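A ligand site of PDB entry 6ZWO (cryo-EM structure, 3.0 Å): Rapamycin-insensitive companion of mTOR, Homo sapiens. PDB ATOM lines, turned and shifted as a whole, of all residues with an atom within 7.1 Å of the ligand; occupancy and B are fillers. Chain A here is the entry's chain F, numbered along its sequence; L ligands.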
ATOM      1  N   VAL A 537     -24.919 -11.721   1.563  1.00  0.00           N
ATOM      2  CA  VAL A 537     -24.852 -10.268   1.507  1.00  0.00           C
ATOM      3  C   VAL A 537     -25.905  -9.719   0.552  1.00  0.00           C
ATOM      4  O   VAL A 537     -26.561  -8.707   0.841  1.00  0.00           O
ATOM      5  CB  VAL A 537     -23.436  -9.806   1.116  1.00  0.00           C
ATOM      6  CG1 VAL A 537     -23.452  -8.356   0.662  1.00  0.00           C
ATOM      7  CG2 VAL A 537     -22.491  -9.969   2.289  1.00  0.00           C
ATOM      8  N   LEU A 538     -26.117 -10.382  -0.579  1.00  0.00           N
ATOM      9  CA  LEU A 538     -27.039  -9.901  -1.596  1.00  0.00           C
ATOM     10  C   LEU A 538     -28.478 -10.346  -1.365  1.00  0.00           C
ATOM     11  O   LEU A 538     -29.396  -9.724  -1.905  1.00  0.00           O
ATOM     12  CB  LEU A 538     -26.581 -10.355  -2.978  1.00  0.00           C
ATOM     13  CG  LEU A 538     -25.191  -9.867  -3.366  1.00  0.00           C
ATOM     14  CD1 LEU A 538     -24.165 -10.968  -3.166  1.00  0.00           C
ATOM     15  CD2 LEU A 538     -25.170  -9.383  -4.808  1.00  0.00           C
ATOM     16  N   LYS A 541     -30.161  -7.110   3.134  1.00  0.00           N
ATOM     17  CA  LYS A 541     -29.254  -6.059   3.549  1.00  0.00           C
ATOM     18  C   LYS A 541     -29.222  -5.864   5.054  1.00  0.00           C
ATOM     19  O   LYS A 541     -28.632  -4.879   5.534  1.00  0.00           O
ATOM     20  CB  LYS A 541     -29.611  -4.739   2.861  1.00  0.00           C
ATOM     21  CG  LYS A 541     -31.064  -4.323   3.058  1.00  0.00           C
ATOM     22  CD  LYS A 541     -31.499  -3.341   1.985  1.00  0.00           C
ATOM     23  CE  LYS A 541     -33.013  -3.270   1.883  1.00  0.00           C
ATOM     24  NZ  LYS A 541     -33.471  -3.002   0.493  1.00  0.00           N
ATOM     25  N   GLU A 542     -29.853  -6.748   5.822  1.00  0.00           N
ATOM     26  CA  GLU A 542     -29.803  -6.652   7.277  1.00  0.00           C
ATOM     27  C   GLU A 542     -28.404  -6.987   7.768  1.00  0.00           C
ATOM     28  O   GLU A 542     -27.905  -8.097   7.531  1.00  0.00           O
ATOM     29  CB  GLU A 542     -30.841  -7.587   7.911  1.00  0.00           C
ATOM     30  CG  GLU A 542     -30.609  -7.875   9.382  1.00  0.00           C
ATOM     31  CD  GLU A 542     -30.804  -6.663  10.267  1.00  0.00           C
ATOM     32  OE1 GLU A 542     -31.912  -6.523  10.843  1.00  0.00           O
ATOM     33  OE2 GLU A 542     -29.870  -5.850  10.393  1.00  0.00           O
ATOM     34  N   ASN A 543     -27.766  -6.045   8.454  1.00  0.00           N
ATOM     35  CA  ASN A 543     -26.409  -6.246   8.922  1.00  0.00           C
ATOM     36  C   ASN A 543     -26.398  -7.171  10.134  1.00  0.00           C
ATOM     37  O   ASN A 543     -27.435  -7.536  10.685  1.00  0.00           O
ATOM     38  CB  ASN A 543     -25.767  -4.906   9.270  1.00  0.00           C
ATOM     39  CG  ASN A 543     -25.607  -4.012   8.061  1.00  0.00           C
ATOM     40  OD1 ASN A 543     -26.068  -2.864   8.054  1.00  0.00           O
ATOM     41  ND2 ASN A 543     -24.947  -4.523   7.036  1.00  0.00           N
ATOM     42  N   TRP A 546     -24.813 -11.386   8.290  1.00  0.00           N
ATOM     43  CA  TRP A 546     -24.077 -11.894   7.147  1.00  0.00           C
ATOM     44  C   TRP A 546     -23.082 -12.959   7.600  1.00  0.00           C
ATOM     45  O   TRP A 546     -22.776 -13.092   8.786  1.00  0.00           O
ATOM     46  CB  TRP A 546     -23.340 -10.758   6.445  1.00  0.00           C
ATOM     47  CG  TRP A 546     -24.220  -9.864   5.632  1.00  0.00           C
ATOM     48  CD1 TRP A 546     -25.432 -10.176   5.086  1.00  0.00           C
ATOM     49  CD2 TRP A 546     -23.961  -8.498   5.273  1.00  0.00           C
ATOM     50  NE1 TRP A 546     -25.940  -9.085   4.412  1.00  0.00           N
ATOM     51  CE2 TRP A 546     -25.049  -8.047   4.517  1.00  0.00           C
ATOM     52  CE3 TRP A 546     -22.904  -7.623   5.527  1.00  0.00           C
ATOM     53  CZ2 TRP A 546     -25.114  -6.757   3.994  1.00  0.00           C
ATOM     54  CZ3 TRP A 546     -22.971  -6.334   5.018  1.00  0.00           C
ATOM     55  CH2 TRP A 546     -24.067  -5.915   4.259  1.00  0.00           C
ATOM     56  N   GLU A 568     -21.758  -7.893 -12.368  1.00  0.00           N
ATOM     57  CA  GLU A 568     -22.612  -6.907 -11.708  1.00  0.00           C
ATOM     58  C   GLU A 568     -22.934  -7.312 -10.281  1.00  0.00           C
ATOM     59  O   GLU A 568     -23.103  -6.450  -9.408  1.00  0.00           O
ATOM     60  CB  GLU A 568     -23.880  -6.700 -12.527  1.00  0.00           C
ATOM     61  CG  GLU A 568     -24.688  -5.451 -12.182  1.00  0.00           C
ATOM     62  CD  GLU A 568     -25.570  -5.629 -10.960  1.00  0.00           C
ATOM     63  OE1 GLU A 568     -25.956  -4.612 -10.359  1.00  0.00           O
ATOM     64  OE2 GLU A 568     -25.883  -6.792 -10.625  1.00  0.00           O
ATOM     65  N   HIS A 571     -20.110  -6.113  -8.146  1.00  0.00           N
ATOM     66  CA  HIS A 571     -20.201  -4.678  -7.911  1.00  0.00           C
ATOM     67  C   HIS A 571     -21.279  -4.352  -6.882  1.00  0.00           C
ATOM     68  O   HIS A 571     -21.099  -3.449  -6.057  1.00  0.00           O
ATOM     69  CB  HIS A 571     -20.455  -3.937  -9.222  1.00  0.00           C
ATOM     70  CG  HIS A 571     -19.281  -3.943 -10.149  1.00  0.00           C
ATOM     71  ND1 HIS A 571     -18.983  -5.015 -10.965  1.00  0.00           N
ATOM     72  CD2 HIS A 571     -18.333  -3.004 -10.396  1.00  0.00           C
ATOM     73  CE1 HIS A 571     -17.894  -4.731 -11.668  1.00  0.00           C
ATOM     74  NE2 HIS A 571     -17.487  -3.524 -11.344  1.00  0.00           N
ATOM     75  N   ARG A 572     -22.411  -5.067  -6.927  1.00  0.00           N
ATOM     76  CA  ARG A 572     -23.419  -4.901  -5.892  1.00  0.00           C
ATOM     77  C   ARG A 572     -22.857  -5.253  -4.517  1.00  0.00           C
ATOM     78  O   ARG A 572     -23.076  -4.523  -3.542  1.00  0.00           O
ATOM     79  CB  ARG A 572     -24.646  -5.754  -6.199  1.00  0.00           C
ATOM     80  CG  ARG A 572     -25.626  -5.142  -7.178  1.00  0.00           C
ATOM     81  CD  ARG A 572     -26.640  -6.160  -7.644  1.00  0.00           C
ATOM     82  NE  ARG A 572     -27.100  -7.015  -6.557  1.00  0.00           N
ATOM     83  CZ  ARG A 572     -28.281  -6.888  -5.963  1.00  0.00           C
ATOM     84  NH1 ARG A 572     -29.132  -5.950  -6.356  1.00  0.00           N
ATOM     85  NH2 ARG A 572     -28.618  -7.701  -4.971  1.00  0.00           N
ATOM     86  N   PHE A 573     -22.139  -6.366  -4.428  1.00  0.00           N
ATOM     87  CA  PHE A 573     -21.490  -6.774  -3.185  1.00  0.00           C
ATOM     88  C   PHE A 573     -20.564  -5.669  -2.666  1.00  0.00           C
ATOM     89  O   PHE A 573     -20.621  -5.297  -1.490  1.00  0.00           O
ATOM     90  CB  PHE A 573     -20.725  -8.071  -3.430  1.00  0.00           C
ATOM     91  CG  PHE A 573     -19.999  -8.617  -2.237  1.00  0.00           C
ATOM     92  CD1 PHE A 573     -20.635  -9.482  -1.369  1.00  0.00           C
ATOM     93  CD2 PHE A 573     -18.675  -8.295  -2.010  1.00  0.00           C
ATOM     94  CE1 PHE A 573     -19.965  -9.997  -0.276  1.00  0.00           C
ATOM     95  CE2 PHE A 573     -18.007  -8.800  -0.917  1.00  0.00           C
ATOM     96  CZ  PHE A 573     -18.652  -9.656  -0.043  1.00  0.00           C
ATOM     97  N   VAL A 574     -19.715  -5.143  -3.547  1.00  0.00           N
ATOM     98  CA  VAL A 574     -18.756  -4.123  -3.154  1.00  0.00           C
ATOM     99  C   VAL A 574     -19.468  -2.858  -2.694  1.00  0.00           C
ATOM    100  O   VAL A 574     -19.084  -2.246  -1.683  1.00  0.00           O
ATOM    101  CB  VAL A 574     -17.779  -3.838  -4.309  1.00  0.00           C
ATOM    102  CG1 VAL A 574     -16.991  -2.563  -4.034  1.00  0.00           C
ATOM    103  CG2 VAL A 574     -16.838  -5.013  -4.511  1.00  0.00           C
ATOM    104  N   ARG A 575     -20.512  -2.450  -3.402  1.00  0.00           N
ATOM    105  CA  ARG A 575     -21.233  -1.227  -3.031  1.00  0.00           C
ATOM    106  C   ARG A 575     -21.959  -1.398  -1.699  1.00  0.00           C
ATOM    107  O   ARG A 575     -21.993  -0.462  -0.884  1.00  0.00           O
ATOM    108  CB  ARG A 575     -22.213  -0.837  -4.131  1.00  0.00           C
ATOM    109  CG  ARG A 575     -21.581  -0.104  -5.303  1.00  0.00           C
ATOM    110  CD  ARG A 575     -22.551   0.064  -6.458  1.00  0.00           C
ATOM    111  NE  ARG A 575     -22.736  -1.174  -7.200  1.00  0.00           N
ATOM    112  CZ  ARG A 575     -23.540  -1.302  -8.253  1.00  0.00           C
ATOM    113  NH1 ARG A 575     -24.225  -0.263  -8.704  1.00  0.00           N
ATOM    114  NH2 ARG A 575     -23.647  -2.466  -8.874  1.00  0.00           N
ATOM    115  N   ARG A 576     -22.533  -2.575  -1.446  1.00  0.00           N
ATOM    116  CA  ARG A 576     -23.197  -2.807  -0.164  1.00  0.00           C
ATOM    117  C   ARG A 576     -22.189  -2.765   0.974  1.00  0.00           C
ATOM    118  O   ARG A 576     -22.444  -2.133   2.012  1.00  0.00           O
ATOM    119  CB  ARG A 576     -23.918  -4.151  -0.181  1.00  0.00           C
ATOM    120  CG  ARG A 576     -25.037  -4.242  -1.208  1.00  0.00           C
ATOM    121  CD  ARG A 576     -26.258  -4.985  -0.688  1.00  0.00           C
ATOM    122  NE  ARG A 576     -27.316  -5.026  -1.690  1.00  0.00           N
ATOM    123  CZ  ARG A 576     -28.444  -5.711  -1.556  1.00  0.00           C
ATOM    124  NH1 ARG A 576     -29.351  -5.694  -2.527  1.00  0.00           N
ATOM    125  NH2 ARG A 576     -28.672  -6.413  -0.458  1.00  0.00           N
ATOM    126  N   LEU A 577     -21.034  -3.405   0.798  1.00  0.00           N
ATOM    127  CA  LEU A 577     -20.019  -3.373   1.858  1.00  0.00           C
ATOM    128  C   LEU A 577     -19.493  -1.952   2.070  1.00  0.00           C
ATOM    129  O   LEU A 577     -19.245  -1.546   3.205  1.00  0.00           O
ATOM    130  CB  LEU A 577     -18.880  -4.320   1.521  1.00  0.00           C
ATOM    131  CG  LEU A 577     -18.932  -5.681   2.225  1.00  0.00           C
ATOM    132  CD1 LEU A 577     -17.816  -6.571   1.736  1.00  0.00           C
ATOM    133  CD2 LEU A 577     -18.866  -5.511   3.734  1.00  0.00           C
ATOM    134  N   LEU A 578     -19.343  -1.192   0.984  1.00  0.00           N
ATOM    135  CA  LEU A 578     -18.891   0.187   1.105  1.00  0.00           C
ATOM    136  C   LEU A 578     -19.891   1.015   1.903  1.00  0.00           C
ATOM    137  O   LEU A 578     -19.506   1.729   2.838  1.00  0.00           O
ATOM    138  CB  LEU A 578     -18.695   0.793  -0.293  1.00  0.00           C
ATOM    139  CG  LEU A 578     -18.397   2.287  -0.385  1.00  0.00           C
ATOM    140  CD1 LEU A 578     -17.304   2.699   0.583  1.00  0.00           C
ATOM    141  CD2 LEU A 578     -18.038   2.679  -1.801  1.00  0.00           C
ATOM    142  N   TYR A 579     -21.171   0.934   1.538  1.00  0.00           N
ATOM    143  CA  TYR A 579     -22.191   1.677   2.274  1.00  0.00           C
ATOM    144  C   TYR A 579     -22.258   1.235   3.731  1.00  0.00           C
ATOM    145  O   TYR A 579     -22.605   2.045   4.604  1.00  0.00           O
ATOM    146  CB  TYR A 579     -23.549   1.523   1.603  1.00  0.00           C
ATOM    147  CG  TYR A 579     -24.659   2.301   2.275  1.00  0.00           C
ATOM    148  CD1 TYR A 579     -24.888   3.633   1.965  1.00  0.00           C
ATOM    149  CD2 TYR A 579     -25.478   1.699   3.231  1.00  0.00           C
ATOM    150  CE1 TYR A 579     -25.905   4.347   2.578  1.00  0.00           C
ATOM    151  CE2 TYR A 579     -26.493   2.403   3.844  1.00  0.00           C
ATOM    152  CZ  TYR A 579     -26.702   3.727   3.508  1.00  0.00           C
ATOM    153  OH  TYR A 579     -27.711   4.432   4.129  1.00  0.00           O
ATOM    154  N   PHE A 580     -21.943  -0.030   4.021  1.00  0.00           N
ATOM    155  CA  PHE A 580     -21.913  -0.465   5.407  1.00  0.00           C
ATOM    156  C   PHE A 580     -20.725   0.137   6.159  1.00  0.00           C
ATOM    157  O   PHE A 580     -20.856   0.527   7.323  1.00  0.00           O
ATOM    158  CB  PHE A 580     -21.886  -1.983   5.489  1.00  0.00           C
ATOM    159  CG  PHE A 580     -21.517  -2.511   6.852  1.00  0.00           C
ATOM    160  CD1 PHE A 580     -22.372  -2.339   7.924  1.00  0.00           C
ATOM    161  CD2 PHE A 580     -20.310  -3.164   7.063  1.00  0.00           C
ATOM    162  CE1 PHE A 580     -22.045  -2.813   9.175  1.00  0.00           C
ATOM    163  CE2 PHE A 580     -19.983  -3.638   8.313  1.00  0.00           C
ATOM    164  CZ  PHE A 580     -20.850  -3.467   9.370  1.00  0.00           C
ATOM    165  N   LYS A 582     -18.919   2.911   5.520  1.00  0.00           N
ATOM    166  CA  LYS A 582     -18.766   4.359   5.577  1.00  0.00           C
ATOM    167  C   LYS A 582     -19.262   4.898   6.913  1.00  0.00           C
ATOM    168  O   LYS A 582     -20.308   4.470   7.403  1.00  0.00           O
ATOM    169  CB  LYS A 582     -19.527   5.021   4.431  1.00  0.00           C
ATOM    170  CG  LYS A 582     -18.849   4.869   3.076  1.00  0.00           C
ATOM    171  CD  LYS A 582     -19.795   5.214   1.944  1.00  0.00           C
ATOM    172  CE  LYS A 582     -20.307   6.637   2.052  1.00  0.00           C
ATOM    173  NZ  LYS A 582     -21.280   6.957   0.980  1.00  0.00           N
ATOM    174  N   SER A 585     -22.877   6.702   6.943  1.00  0.00           N
ATOM    175  CA  SER A 585     -24.060   5.845   7.014  1.00  0.00           C
ATOM    176  C   SER A 585     -24.409   5.465   8.446  1.00  0.00           C
ATOM    177  O   SER A 585     -25.538   5.024   8.688  1.00  0.00           O
ATOM    178  CB  SER A 585     -23.836   4.597   6.175  1.00  0.00           C
ATOM    179  OG  SER A 585     -23.053   3.646   6.879  1.00  0.00           O
ATOM    180  N   LEU A 587     -23.419   2.974  10.410  1.00  0.00           N
ATOM    181  CA  LEU A 587     -23.688   1.545  10.572  1.00  0.00           C
ATOM    182  C   LEU A 587     -22.550   0.819  11.264  1.00  0.00           C
ATOM    183  O   LEU A 587     -22.792   0.104  12.237  1.00  0.00           O
ATOM    184  CB  LEU A 587     -23.962   0.912   9.197  1.00  0.00           C
ATOM    185  CG  LEU A 587     -25.290   1.291   8.525  1.00  0.00           C
ATOM    186  CD1 LEU A 587     -25.174   1.163   7.015  1.00  0.00           C
ATOM    187  CD2 LEU A 587     -26.419   0.432   9.055  1.00  0.00           C
HETATM  188  P1  LIG L   1     -31.195  -1.362  -4.235  1.00  0.00           P
HETATM  189  S1  LIG L   1     -31.248  -0.038  -5.628  1.00  0.00           S
HETATM  190  O1  LIG L   1     -31.962  -2.673  -4.794  1.00  0.00           O
HETATM  191  O2  LIG L   1     -31.776  -0.909  -2.950  1.00  0.00           O
HETATM  192  P2  LIG L   1     -29.011  -2.897  -5.085  1.00  0.00           P
HETATM  193  O3  LIG L   1     -29.152  -2.370  -6.464  1.00  0.00           O
HETATM  194  O4  LIG L   1     -29.559  -4.222  -4.732  1.00  0.00           O
HETATM  195  O5  LIG L   1     -29.653  -1.814  -4.069  1.00  0.00           O
HETATM  196  P3  LIG L   1     -26.769  -1.502  -4.154  1.00  0.00           P
HETATM  197  O6  LIG L   1     -27.362  -0.365  -4.896  1.00  0.00           O
HETATM  198  O7  LIG L   1     -25.306  -1.703  -4.186  1.00  0.00           O
HETATM  199  O8  LIG L   1     -27.453  -2.859  -4.681  1.00  0.00           O
HETATM  200  O9  LIG L   1     -27.244  -1.457  -2.622  1.00  0.00           O
HETATM  201  C1  LIG L   1     -26.585  -0.603  -1.691  1.00  0.00           C
HETATM  202  C2  LIG L   1     -27.618   0.310  -1.017  1.00  0.00           C
HETATM  203  O10 LIG L   1     -28.511  -0.417  -0.141  1.00  0.00           O
HETATM  204  C3  LIG L   1     -26.963   1.224  -0.029  1.00  0.00           C
HETATM  205  O11 LIG L   1     -26.114   2.167  -0.676  1.00  0.00           O
HETATM  206  C4  LIG L   1     -28.246   1.862   0.414  1.00  0.00           C
HETATM  207  O12 LIG L   1     -28.833   2.483  -0.728  1.00  0.00           O
HETATM  208  C5  LIG L   1     -29.032   0.606   0.769  1.00  0.00           C
HETATM  209  N1  LIG L   1     -28.814   0.164   2.169  1.00  0.00           N
HETATM  210  C6  LIG L   1     -29.627   0.537   3.161  1.00  0.00           C
HETATM  211  N2  LIG L   1     -29.180  -0.018   4.284  1.00  0.00           N
HETATM  212  C7  LIG L   1     -28.092  -0.720   4.003  1.00  0.00           C
HETATM  213  C8  LIG L   1     -27.286  -1.444   4.774  1.00  0.00           C
HETATM  214  N3  LIG L   1     -27.599  -1.492   6.064  1.00  0.00           N
HETATM  215  N4  LIG L   1     -26.219  -2.088   4.278  1.00  0.00           N
HETATM  216  C9  LIG L   1     -25.959  -1.999   2.910  1.00  0.00           C
HETATM  217  N5  LIG L   1     -26.813  -1.232   2.119  1.00  0.00           N
HETATM  218  C10 LIG L   1     -27.866  -0.606   2.681  1.00  0.00           C
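O4 of the ligand is in salt-bridge range of NH1 of Arg 572, at 2.4 Å.
NH1 of Arg 576 lies within salt-bridge range of O4 of the ligand.
OD1 of Asn 543 lies within hydrogen-bond range of N3 of the ligand.
O7 of the ligand lies within salt-bridge range of NE of Arg 575 (3.996 Å).
The backbone carbonyl oxygen (O) of Val 537 sits at hydrogen-bond distance from the guanidinium group (NH2) of Arg 576 (3.4 Å).
The guanidinium group (NE) of Arg 575 is in hydrogen-bond range of the backbone carbonyl oxygen (O) of His 571 (3.0 Å).
The guanidinium group (NH2) of Arg 575 is in salt-bridge range of the side-chain carboxylate (OE1) of Glu 568 (3.5 Å).
The backbone carbonyl oxygen (O) of Tyr 579 sits at hydrogen-bond distance from the side-chain hydroxyl (OG) of Ser 585 (2.8 Å).
Merely in contact with the ligand: Lys 541, Tyr 579 and Leu 587.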
